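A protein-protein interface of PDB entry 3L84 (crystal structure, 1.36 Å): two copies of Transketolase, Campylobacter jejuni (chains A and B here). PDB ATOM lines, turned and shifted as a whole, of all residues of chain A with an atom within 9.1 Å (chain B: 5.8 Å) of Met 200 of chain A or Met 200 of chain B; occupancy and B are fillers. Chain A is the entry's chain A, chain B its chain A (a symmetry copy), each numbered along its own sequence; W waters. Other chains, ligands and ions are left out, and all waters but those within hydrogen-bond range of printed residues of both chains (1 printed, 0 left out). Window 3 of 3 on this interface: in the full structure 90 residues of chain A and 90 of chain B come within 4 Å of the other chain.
SD of Met 200 of chain A is in hydrogen-bond range of N of Ala 204 of chain B, 3.6 Å away. The side-chain carboxylate (OE2) of Glu 196 of chain A sits at hydrogen-bond distance from the side-chain amide nitrogen (NE2) of Gln 205 of chain B, 3.0 Å away. The backbone NH (N) of Asn 197 of chain A sits at hydrogen-bond distance from the backbone carbonyl oxygen (O) of Ala 204 of chain B. SD of Met 200 of chain B sits close to O of Met 200 of chain A. The side-chain sulfur of Met 200 of chain B sits at hydrogen-bond distance from the backbone NH of Ala 204 of chain A, at 3.6 Å. The backbone NH (N) of Asn 197 of chain B sits at hydrogen-bond distance from the backbone carbonyl oxygen (O) of Ala 204 of chain A (3.0 Å).
NZ of Lys 199 of chain A lies within salt-bridge range of OE1 of Glu 203 of chain A (2.8 Å). The side-chain amide oxygen (OD1) of Asn 197 of chain A sits at hydrogen-bond distance from the backbone NH (N) of Met 200 of chain A (3.0 Å). OD1 of Asn 197 of chain A sits close to N of Lys 199 of chain A (3.3 Å). The backbone NH of Met 200 of chain B sits at hydrogen-bond distance from the side-chain amide oxygen of Asn 197 of chain B (3.0 Å). NZ of Lys 199 of chain B is in salt-bridge range of OE1 of Glu 203 of chain B (2.8 Å). The side-chain carboxylate of Glu 196 of chain A is in salt-bridge range of the guanidinium group of Arg 201 of chain A (3.0 Å).
Among the printed residues, merely in contact across the chains: Glu 196 of chain A with Ala 204 of chain B (3.5 Å), Met 200 of chain A with Glu 203 of chain B (3.8 Å), Arg 201 of chain A with Ala 204 of chain B (3.4 Å), Glu 203 of chain A with Met 200 of chain B (3.8 Å) and Ala 204 of chain A with Arg 201 of chain B (3.4 Å).
Met 200 of chain A touches just these residues of chain B: Met 200, Glu 203 and Ala 204. Met 200 of chain B touches three residues of chain A. Of the printed residues of chain B, Glu 196 of chain A touches Ala 204 (3.5 Å) and Gln 205 (3.0 Å). Of the printed residues of chain A, Glu 203 of chain B touches Met 200. Of the printed residues of chain B, Arg 201 of chain A touches Ala 204 (3.4 Å). Of the printed residues of chain B, Glu 203 of chain A touches Met 200. Of the printed residues of chain A, Ala 204 of chain B touches Glu 196 (3.5 Å), Asn 197 (3.0 Å), Met 200 (3.6 Å) and Arg 201 (3.4 Å). Lys 199 of chain A touches none of the printed residues of chain B. Phe 202 of chain B touches none of the printed residues of chain A.
Printed residues of chain A that touch a printed residue of chain B: Glu 196, Asn 197, Met 200, Arg 201, Glu 203 and Ala 204. Of the 9 printed residues of chain B, 6 touch a printed residue of chain A. Hydrophobic or aromatic side chains of chain B that line the printed part of chain A: Met 200 and Ala 204. Among the printed residues, no Asp or Glu carboxylate lies within 4 Å of a Lys or Arg side-chain nitrogen of the other chain.
Asn 197 of chain A touches Ala 204 of chain B, and with the chains exchanged Ala 204 of chain A touches Asn 197 of chain B. Met 200 of chain B touches its own counterpart, Met 200 of chain A. Met 200 of chain A touches Ala 204 of chain B, and with the chains exchanged Ala 204 of chain A touches Met 200 of chain B. Arg 201 of chain A touches Ala 204 of chain B, and with the chains exchanged Ala 204 of chain A touches Arg 201 of chain B. Positions printed for both chains: 197, 198, 199, 200, 201, 202, 203, 204 and 205. Of the 11 pairs that touch across the chains among the printed residues, 9 have their exchanged pair printed and touching as well.
Water W1 bridges the backbone carbonyl oxygen of Asn 195 of chain A (3.1 Å) and the backbone carbonyl oxygen of Ala 204 of chain B (3.4 Å).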
ATOM      1  N   ASN A 195      11.556  -8.688  30.532  1.00  0.00           N
ATOM      2  CA  ASN A 195      12.843  -7.981  30.674  1.00  0.00           C
ATOM      3  C   ASN A 195      13.766  -8.203  29.470  1.00  0.00           C
ATOM      4  O   ASN A 195      14.991  -8.119  29.615  1.00  0.00           O
ATOM      5  CB  ASN A 195      13.542  -8.346  31.994  1.00  0.00           C
ATOM      6  CG  ASN A 195      14.161  -9.709  31.984  1.00  0.00           C
ATOM      7  OD1 ASN A 195      13.803 -10.571  31.190  1.00  0.00           O
ATOM      8  ND2 ASN A 195      15.118  -9.933  32.896  1.00  0.00           N
ATOM      9  N   GLU A 196      13.213  -8.411  28.294  1.00  0.00           N
ATOM     10  CA  GLU A 196      13.996  -8.554  27.059  1.00  0.00           C
ATOM     11  C   GLU A 196      14.825  -7.315  26.787  1.00  0.00           C
ATOM     12  O   GLU A 196      14.421  -6.196  27.128  1.00  0.00           O
ATOM     13  CB  GLU A 196      13.105  -8.745  25.822  1.00  0.00           C
ATOM     14  CG  GLU A 196      12.275  -9.973  25.886  1.00  0.00           C
ATOM     15  CD  GLU A 196      11.454 -10.219  24.636  1.00  0.00           C
ATOM     16  OE1 GLU A 196      11.403  -9.368  23.734  1.00  0.00           O
ATOM     17  OE2 GLU A 196      10.807 -11.300  24.597  1.00  0.00           O
ATOM     18  N   ASN A 197      15.966  -7.528  26.135  1.00  0.00           N
ATOM     19  CA  ASN A 197      16.709  -6.448  25.507  1.00  0.00           C
ATOM     20  C   ASN A 197      16.008  -6.177  24.173  1.00  0.00           C
ATOM     21  O   ASN A 197      16.218  -6.873  23.175  1.00  0.00           O
ATOM     22  CB  ASN A 197      18.173  -6.837  25.344  1.00  0.00           C
ATOM     23  CG  ASN A 197      19.003  -5.710  24.784  1.00  0.00           C
ATOM     24  OD1 ASN A 197      18.500  -4.870  24.034  1.00  0.00           O
ATOM     25  ND2 ASN A 197      20.273  -5.689  25.148  1.00  0.00           N
ATOM     26  N   VAL A 198      15.113  -5.190  24.181  1.00  0.00           N
ATOM     27  CA  VAL A 198      14.251  -4.918  23.040  1.00  0.00           C
ATOM     28  C   VAL A 198      15.071  -4.452  21.826  1.00  0.00           C
ATOM     29  O   VAL A 198      14.797  -4.874  20.701  1.00  0.00           O
ATOM     30  CB  VAL A 198      13.137  -3.903  23.413  1.00  0.00           C
ATOM     31  CG1 VAL A 198      12.328  -3.454  22.150  1.00  0.00           C
ATOM     32  CG2 VAL A 198      12.209  -4.531  24.481  1.00  0.00           C
ATOM     33  N   LYS A 199      16.109  -3.635  22.059  1.00  0.00           N
ATOM     34  CA  LYS A 199      16.969  -3.223  20.962  1.00  0.00           C
ATOM     35  C   LYS A 199      17.608  -4.438  20.274  1.00  0.00           C
ATOM     36  O   LYS A 199      17.561  -4.571  19.054  1.00  0.00           O
ATOM     37  CB  LYS A 199      18.020  -2.250  21.477  1.00  0.00           C
ATOM     38  CG  LYS A 199      19.031  -1.770  20.452  1.00  0.00           C
ATOM     39  CD  LYS A 199      19.833  -0.591  21.034  1.00  0.00           C
ATOM     40  CE  LYS A 199      20.642   0.103  19.977  1.00  0.00           C
ATOM     41  NZ  LYS A 199      21.822  -0.687  19.600  1.00  0.00           N
ATOM     42  N   MET A 200      18.170  -5.347  21.069  1.00  0.00           N
ATOM     43  CA  MET A 200      18.769  -6.540  20.504  1.00  0.00           C
ATOM     44  C   MET A 200      17.790  -7.452  19.776  1.00  0.00           C
ATOM     45  O   MET A 200      18.108  -8.013  18.706  1.00  0.00           O
ATOM     46  CB  MET A 200      19.486  -7.335  21.595  1.00  0.00           C
ATOM     47  CG  MET A 200      20.368  -8.444  21.097  1.00  0.00           C
ATOM     48  SD  MET A 200      21.369  -9.333  22.471  1.00  0.00           S
ATOM     49  CE  MET A 200      21.522  -8.068  23.761  1.00  0.00           C
ATOM     50  N   ARG A 201      16.585  -7.602  20.336  1.00  0.00           N
ATOM     51  CA  ARG A 201      15.542  -8.388  19.715  1.00  0.00           C
ATOM     52  C   ARG A 201      15.251  -7.881  18.322  1.00  0.00           C
ATOM     53  O   ARG A 201      15.184  -8.664  17.367  1.00  0.00           O
ATOM     54  CB  ARG A 201      14.285  -8.286  20.573  1.00  0.00           C
ATOM     55  CG  ARG A 201      12.970  -8.616  19.891  1.00  0.00           C
ATOM     56  CD  ARG A 201      11.813  -8.254  20.774  1.00  0.00           C
ATOM     57  NE  ARG A 201      10.555  -8.369  20.057  1.00  0.00           N
ATOM     58  CZ  ARG A 201       9.362  -8.384  20.635  1.00  0.00           C
ATOM     59  NH1 ARG A 201       9.241  -8.359  21.969  1.00  0.00           N
ATOM     60  NH2 ARG A 201       8.259  -8.406  19.880  1.00  0.00           N
ATOM     61  N   PHE A 202      15.060  -6.564  18.206  1.00  0.00           N
ATOM     62  CA  PHE A 202      14.695  -6.011  16.901  1.00  0.00           C
ATOM     63  C   PHE A 202      15.866  -5.930  15.927  1.00  0.00           C
ATOM     64  O   PHE A 202      15.691  -6.112  14.722  1.00  0.00           O
ATOM     65  CB  PHE A 202      14.010  -4.656  17.069  1.00  0.00           C
ATOM     66  CG  PHE A 202      12.536  -4.776  17.399  1.00  0.00           C
ATOM     67  CD1 PHE A 202      12.118  -4.998  18.689  1.00  0.00           C
ATOM     68  CD2 PHE A 202      11.590  -4.636  16.414  1.00  0.00           C
ATOM     69  CE1 PHE A 202      10.770  -5.122  18.992  1.00  0.00           C
ATOM     70  CE2 PHE A 202      10.252  -4.754  16.704  1.00  0.00           C
ATOM     71  CZ  PHE A 202       9.847  -4.997  18.015  1.00  0.00           C
ATOM     72  N   GLU A 203      17.075  -5.698  16.450  1.00  0.00           N
ATOM     73  CA  GLU A 203      18.245  -5.788  15.591  1.00  0.00           C
ATOM     74  C   GLU A 203      18.442  -7.205  15.049  1.00  0.00           C
ATOM     75  O   GLU A 203      18.832  -7.391  13.896  1.00  0.00           O
ATOM     76  CB  GLU A 203      19.499  -5.290  16.332  1.00  0.00           C
ATOM     77  CG  GLU A 203      19.453  -3.756  16.536  1.00  0.00           C
ATOM     78  CD  GLU A 203      20.636  -3.168  17.299  1.00  0.00           C
ATOM     79  OE1 GLU A 203      20.763  -1.910  17.298  1.00  0.00           O
ATOM     80  OE2 GLU A 203      21.436  -3.909  17.912  1.00  0.00           O
ATOM     81  N   ALA A 204      18.076  -8.222  15.835  1.00  0.00           N
ATOM     82  CA  ALA A 204      18.160  -9.622  15.380  1.00  0.00           C
ATOM     83  C   ALA A 204      17.205  -9.889  14.218  1.00  0.00           C
ATOM     84  O   ALA A 204      17.445 -10.777  13.396  1.00  0.00           O
ATOM     85  CB  ALA A 204      17.860 -10.582  16.528  1.00  0.00           C
ATOM     86  N   GLN A 205      16.149  -9.089  14.130  1.00  0.00           N
ATOM     87  CA  GLN A 205      15.148  -9.181  13.080  1.00  0.00           C
ATOM     88  C   GLN A 205      15.312  -8.109  12.020  1.00  0.00           C
ATOM     89  O   GLN A 205      14.356  -7.809  11.295  1.00  0.00           O
ATOM     90  CB  GLN A 205      13.734  -9.106  13.673  1.00  0.00           C
ATOM     91  CG  GLN A 205      13.429 -10.220  14.602  1.00  0.00           C
ATOM     92  CD  GLN A 205      11.983 -10.238  15.051  1.00  0.00           C
ATOM     93  OE1 GLN A 205      11.451  -9.209  15.460  1.00  0.00           O
ATOM     94  NE2 GLN A 205      11.324 -11.399  14.987  1.00  0.00           N
ATOM     95  N   GLY A 206      16.496  -7.506  11.913  1.00  0.00           N
ATOM     96  CA  GLY A 206      16.813  -6.628  10.807  1.00  0.00           C
ATOM     97  C   GLY A 206      16.282  -5.218  10.875  1.00  0.00           C
ATOM     98  O   GLY A 206      16.183  -4.575   9.836  1.00  0.00           O
ATOM     99  N   PHE A 207      15.989  -4.734  12.077  1.00  0.00           N
ATOM    100  CA  PHE A 207      15.556  -3.356  12.262  1.00  0.00           C
ATOM    101  C   PHE A 207      16.719  -2.427  12.643  1.00  0.00           C
ATOM    102  O   PHE A 207      17.715  -2.836  13.267  1.00  0.00           O
ATOM    103  CB  PHE A 207      14.548  -3.245  13.414  1.00  0.00           C
ATOM    104  CG  PHE A 207      13.132  -3.697  13.079  1.00  0.00           C
ATOM    105  CD1 PHE A 207      12.853  -5.007  12.728  1.00  0.00           C
ATOM    106  CD2 PHE A 207      12.057  -2.821  13.209  1.00  0.00           C
ATOM    107  CE1 PHE A 207      11.547  -5.403  12.443  1.00  0.00           C
ATOM    108  CE2 PHE A 207      10.773  -3.209  12.960  1.00  0.00           C
ATOM    109  CZ  PHE A 207      10.509  -4.499  12.574  1.00  0.00           C
ATOM    110  N   VAL A 209      17.231   0.585  15.279  1.00  0.00           N
ATOM    111  CA  VAL A 209      16.585   0.895  16.540  1.00  0.00           C
ATOM    112  C   VAL A 209      17.059   2.229  17.122  1.00  0.00           C
ATOM    113  O   VAL A 209      18.259   2.412  17.331  1.00  0.00           O
ATOM    114  CB  VAL A 209      16.786  -0.227  17.572  1.00  0.00           C
ATOM    115  CG1 VAL A 209      16.083   0.178  18.884  1.00  0.00           C
ATOM    116  CG2 VAL A 209      16.273  -1.585  17.031  1.00  0.00           C
ATOM    117  N   SER A 211      16.323   5.174  20.291  1.00  0.00           N
ATOM    118  CA  SER A 211      15.820   5.260  21.649  1.00  0.00           C
ATOM    119  C   SER A 211      15.752   6.709  22.073  1.00  0.00           C
ATOM    120  O   SER A 211      16.797   7.410  22.038  1.00  0.00           O
ATOM    121  CB  SER A 211      16.748   4.509  22.598  1.00  0.00           C
ATOM    122  OG  SER A 211      16.747   3.114  22.270  1.00  0.00           O
ATOM    123  N   LEU A 235      12.480   0.843  14.448  1.00  0.00           N
ATOM    124  CA  LEU A 235      11.831   0.885  15.739  1.00  0.00           C
ATOM    125  C   LEU A 235      12.318   2.101  16.482  1.00  0.00           C
ATOM    126  O   LEU A 235      13.520   2.278  16.626  1.00  0.00           O
ATOM    127  CB  LEU A 235      12.138  -0.371  16.550  1.00  0.00           C
ATOM    128  CG  LEU A 235      11.643  -0.356  18.002  1.00  0.00           C
ATOM    129  CD1 LEU A 235      10.123  -0.455  18.017  1.00  0.00           C
ATOM    130  CD2 LEU A 235      12.223  -1.479  18.852  1.00  0.00           C
ATOM    131  N   ILE A 237      12.069   3.359  20.193  1.00  0.00           N
ATOM    132  CA  ILE A 237      11.704   3.047  21.573  1.00  0.00           C
ATOM    133  C   ILE A 237      11.547   4.371  22.294  1.00  0.00           C
ATOM    134  O   ILE A 237      12.542   5.073  22.556  1.00  0.00           O
ATOM    135  CB  ILE A 237      12.775   2.191  22.269  1.00  0.00           C
ATOM    136  CG1 ILE A 237      13.036   0.897  21.486  1.00  0.00           C
ATOM    137  CG2 ILE A 237      12.381   1.883  23.706  1.00  0.00           C
ATOM    138  CD1 ILE A 237      14.137   0.013  22.097  1.00  0.00           C
ATOM    139  N   ASN B 197      18.919 -13.303  12.924  1.00  0.00           N
ATOM    140  CA  ASN B 197      20.112 -13.665  13.671  1.00  0.00           C
ATOM    141  C   ASN B 197      19.618 -14.379  14.931  1.00  0.00           C
ATOM    142  O   ASN B 197      19.215 -13.754  15.917  1.00  0.00           O
ATOM    143  CB  ASN B 197      20.943 -12.424  13.974  1.00  0.00           C
ATOM    144  CG  ASN B 197      22.240 -12.763  14.664  1.00  0.00           C
ATOM    145  OD1 ASN B 197      22.327 -13.757  15.389  1.00  0.00           O
ATOM    146  ND2 ASN B 197      23.248 -11.939  14.440  1.00  0.00           N
ATOM    147  N   VAL B 198      19.586 -15.710  14.866  1.00  0.00           N
ATOM    148  CA  VAL B 198      18.992 -16.522  15.918  1.00  0.00           C
ATOM    149  C   VAL B 198      19.782 -16.391  17.230  1.00  0.00           C
ATOM    150  O   VAL B 198      19.180 -16.293  18.302  1.00  0.00           O
ATOM    151  CB  VAL B 198      18.854 -18.001  15.468  1.00  0.00           C
ATOM    152  CG1 VAL B 198      18.401 -18.918  16.654  1.00  0.00           C
ATOM    153  CG2 VAL B 198      17.862 -18.085  14.282  1.00  0.00           C
ATOM    154  N   LYS B 199      21.118 -16.327  17.143  1.00  0.00           N
ATOM    155  CA  LYS B 199      21.915 -16.125  18.342  1.00  0.00           C
ATOM    156  C   LYS B 199      21.532 -14.814  19.046  1.00  0.00           C
ATOM    157  O   LYS B 199      21.279 -14.793  20.247  1.00  0.00           O
ATOM    158  CB  LYS B 199      23.393 -16.159  17.982  1.00  0.00           C
ATOM    159  CG  LYS B 199      24.355 -15.907  19.128  1.00  0.00           C
ATOM    160  CD  LYS B 199      25.788 -16.257  18.683  1.00  0.00           C
ATOM    161  CE  LYS B 199      26.735 -16.300  19.848  1.00  0.00           C
ATOM    162  NZ  LYS B 199      27.068 -14.949  20.317  1.00  0.00           N
ATOM    163  N   MET B 200      21.449 -13.727  18.280  1.00  0.00           N
ATOM    164  CA  MET B 200      21.064 -12.455  18.858  1.00  0.00           C
ATOM    165  C   MET B 200      19.656 -12.429  19.440  1.00  0.00           C
ATOM    166  O   MET B 200      19.416 -11.839  20.515  1.00  0.00           O
ATOM    167  CB  MET B 200      21.204 -11.342  17.820  1.00  0.00           C
ATOM    168  CG  MET B 200      21.093  -9.947  18.365  1.00  0.00           C
ATOM    169  SD  MET B 200      21.416  -8.567  17.072  1.00  0.00           S
ATOM    170  CE  MET B 200      22.492  -9.376  15.858  1.00  0.00           C
ATOM    171  N   ARG B 201      18.713 -13.076  18.748  1.00  0.00           N
ATOM    172  CA  ARG B 201      17.350 -13.181  19.221  1.00  0.00           C
ATOM    173  C   ARG B 201      17.312 -13.811  20.594  1.00  0.00           C
ATOM    174  O   ARG B 201      16.649 -13.298  21.504  1.00  0.00           O
ATOM    175  CB  ARG B 201      16.563 -14.042  18.238  1.00  0.00           C
ATOM    176  CG  ARG B 201      15.286 -14.674  18.761  1.00  0.00           C
ATOM    177  CD  ARG B 201      14.745 -15.665  17.773  1.00  0.00           C
ATOM    178  NE  ARG B 201      13.648 -16.424  18.347  1.00  0.00           N
ATOM    179  CZ  ARG B 201      12.802 -17.165  17.643  1.00  0.00           C
ATOM    180  NH1 ARG B 201      12.871 -17.209  16.306  1.00  0.00           N
ATOM    181  NH2 ARG B 201      11.878 -17.895  18.273  1.00  0.00           N
ATOM    182  N   PHE B 202      18.011 -14.939  20.742  1.00  0.00           N
ATOM    183  CA  PHE B 202      17.956 -15.648  22.020  1.00  0.00           C
ATOM    184  C   PHE B 202      18.784 -14.987  23.117  1.00  0.00           C
ATOM    185  O   PHE B 202      18.405 -15.011  24.289  1.00  0.00           O
ATOM    186  CB  PHE B 202      18.339 -17.115  21.834  1.00  0.00           C
ATOM    187  CG  PHE B 202      17.188 -17.969  21.343  1.00  0.00           C
ATOM    188  CD1 PHE B 202      16.868 -18.020  20.008  1.00  0.00           C
ATOM    189  CD2 PHE B 202      16.461 -18.730  22.226  1.00  0.00           C
ATOM    190  CE1 PHE B 202      15.805 -18.791  19.557  1.00  0.00           C
ATOM    191  CE2 PHE B 202      15.409 -19.498  21.789  1.00  0.00           C
ATOM    192  CZ  PHE B 202      15.087 -19.524  20.434  1.00  0.00           C
ATOM    193  N   GLU B 203      19.901 -14.357  22.737  1.00  0.00           N
ATOM    194  CA  GLU B 203      20.631 -13.562  23.712  1.00  0.00           C
ATOM    195  C   GLU B 203      19.799 -12.380  24.216  1.00  0.00           C
ATOM    196  O   GLU B 203      19.848 -12.032  25.396  1.00  0.00           O
ATOM    197  CB  GLU B 203      21.977 -13.096  23.131  1.00  0.00           C
ATOM    198  CG  GLU B 203      22.961 -14.281  22.984  1.00  0.00           C
ATOM    199  CD  GLU B 203      24.315 -13.929  22.377  1.00  0.00           C
ATOM    200  OE1 GLU B 203      25.229 -14.801  22.442  1.00  0.00           O
ATOM    201  OE2 GLU B 203      24.502 -12.822  21.824  1.00  0.00           O
ATOM    202  N   ALA B 204      18.947 -11.815  23.355  1.00  0.00           N
ATOM    203  CA  ALA B 204      18.052 -10.716  23.760  1.00  0.00           C
ATOM    204  C   ALA B 204      17.035 -11.181  24.801  1.00  0.00           C
ATOM    205  O   ALA B 204      16.550 -10.383  25.608  1.00  0.00           O
ATOM    206  CB  ALA B 204      17.326 -10.137  22.549  1.00  0.00           C
ATOM    207  N   GLN B 205      16.751 -12.478  24.806  1.00  0.00           N
ATOM    208  CA  GLN B 205      15.826 -13.101  25.738  1.00  0.00           C
ATOM    209  C   GLN B 205      16.531 -13.850  26.852  1.00  0.00           C
ATOM    210  O   GLN B 205      15.929 -14.728  27.481  1.00  0.00           O
ATOM    211  CB  GLN B 205      14.874 -14.053  25.000  1.00  0.00           C
ATOM    212  CG  GLN B 205      14.020 -13.369  24.000  1.00  0.00           C
ATOM    213  CD  GLN B 205      12.969 -14.277  23.398  1.00  0.00           C
ATOM    214  OE1 GLN B 205      13.282 -15.387  22.976  1.00  0.00           O
ATOM    215  NE2 GLN B 205      11.712 -13.827  23.344  1.00  0.00           N
HETATM  216  O   HOH W   1      17.220 -10.108  28.956  1.00  0.00           O
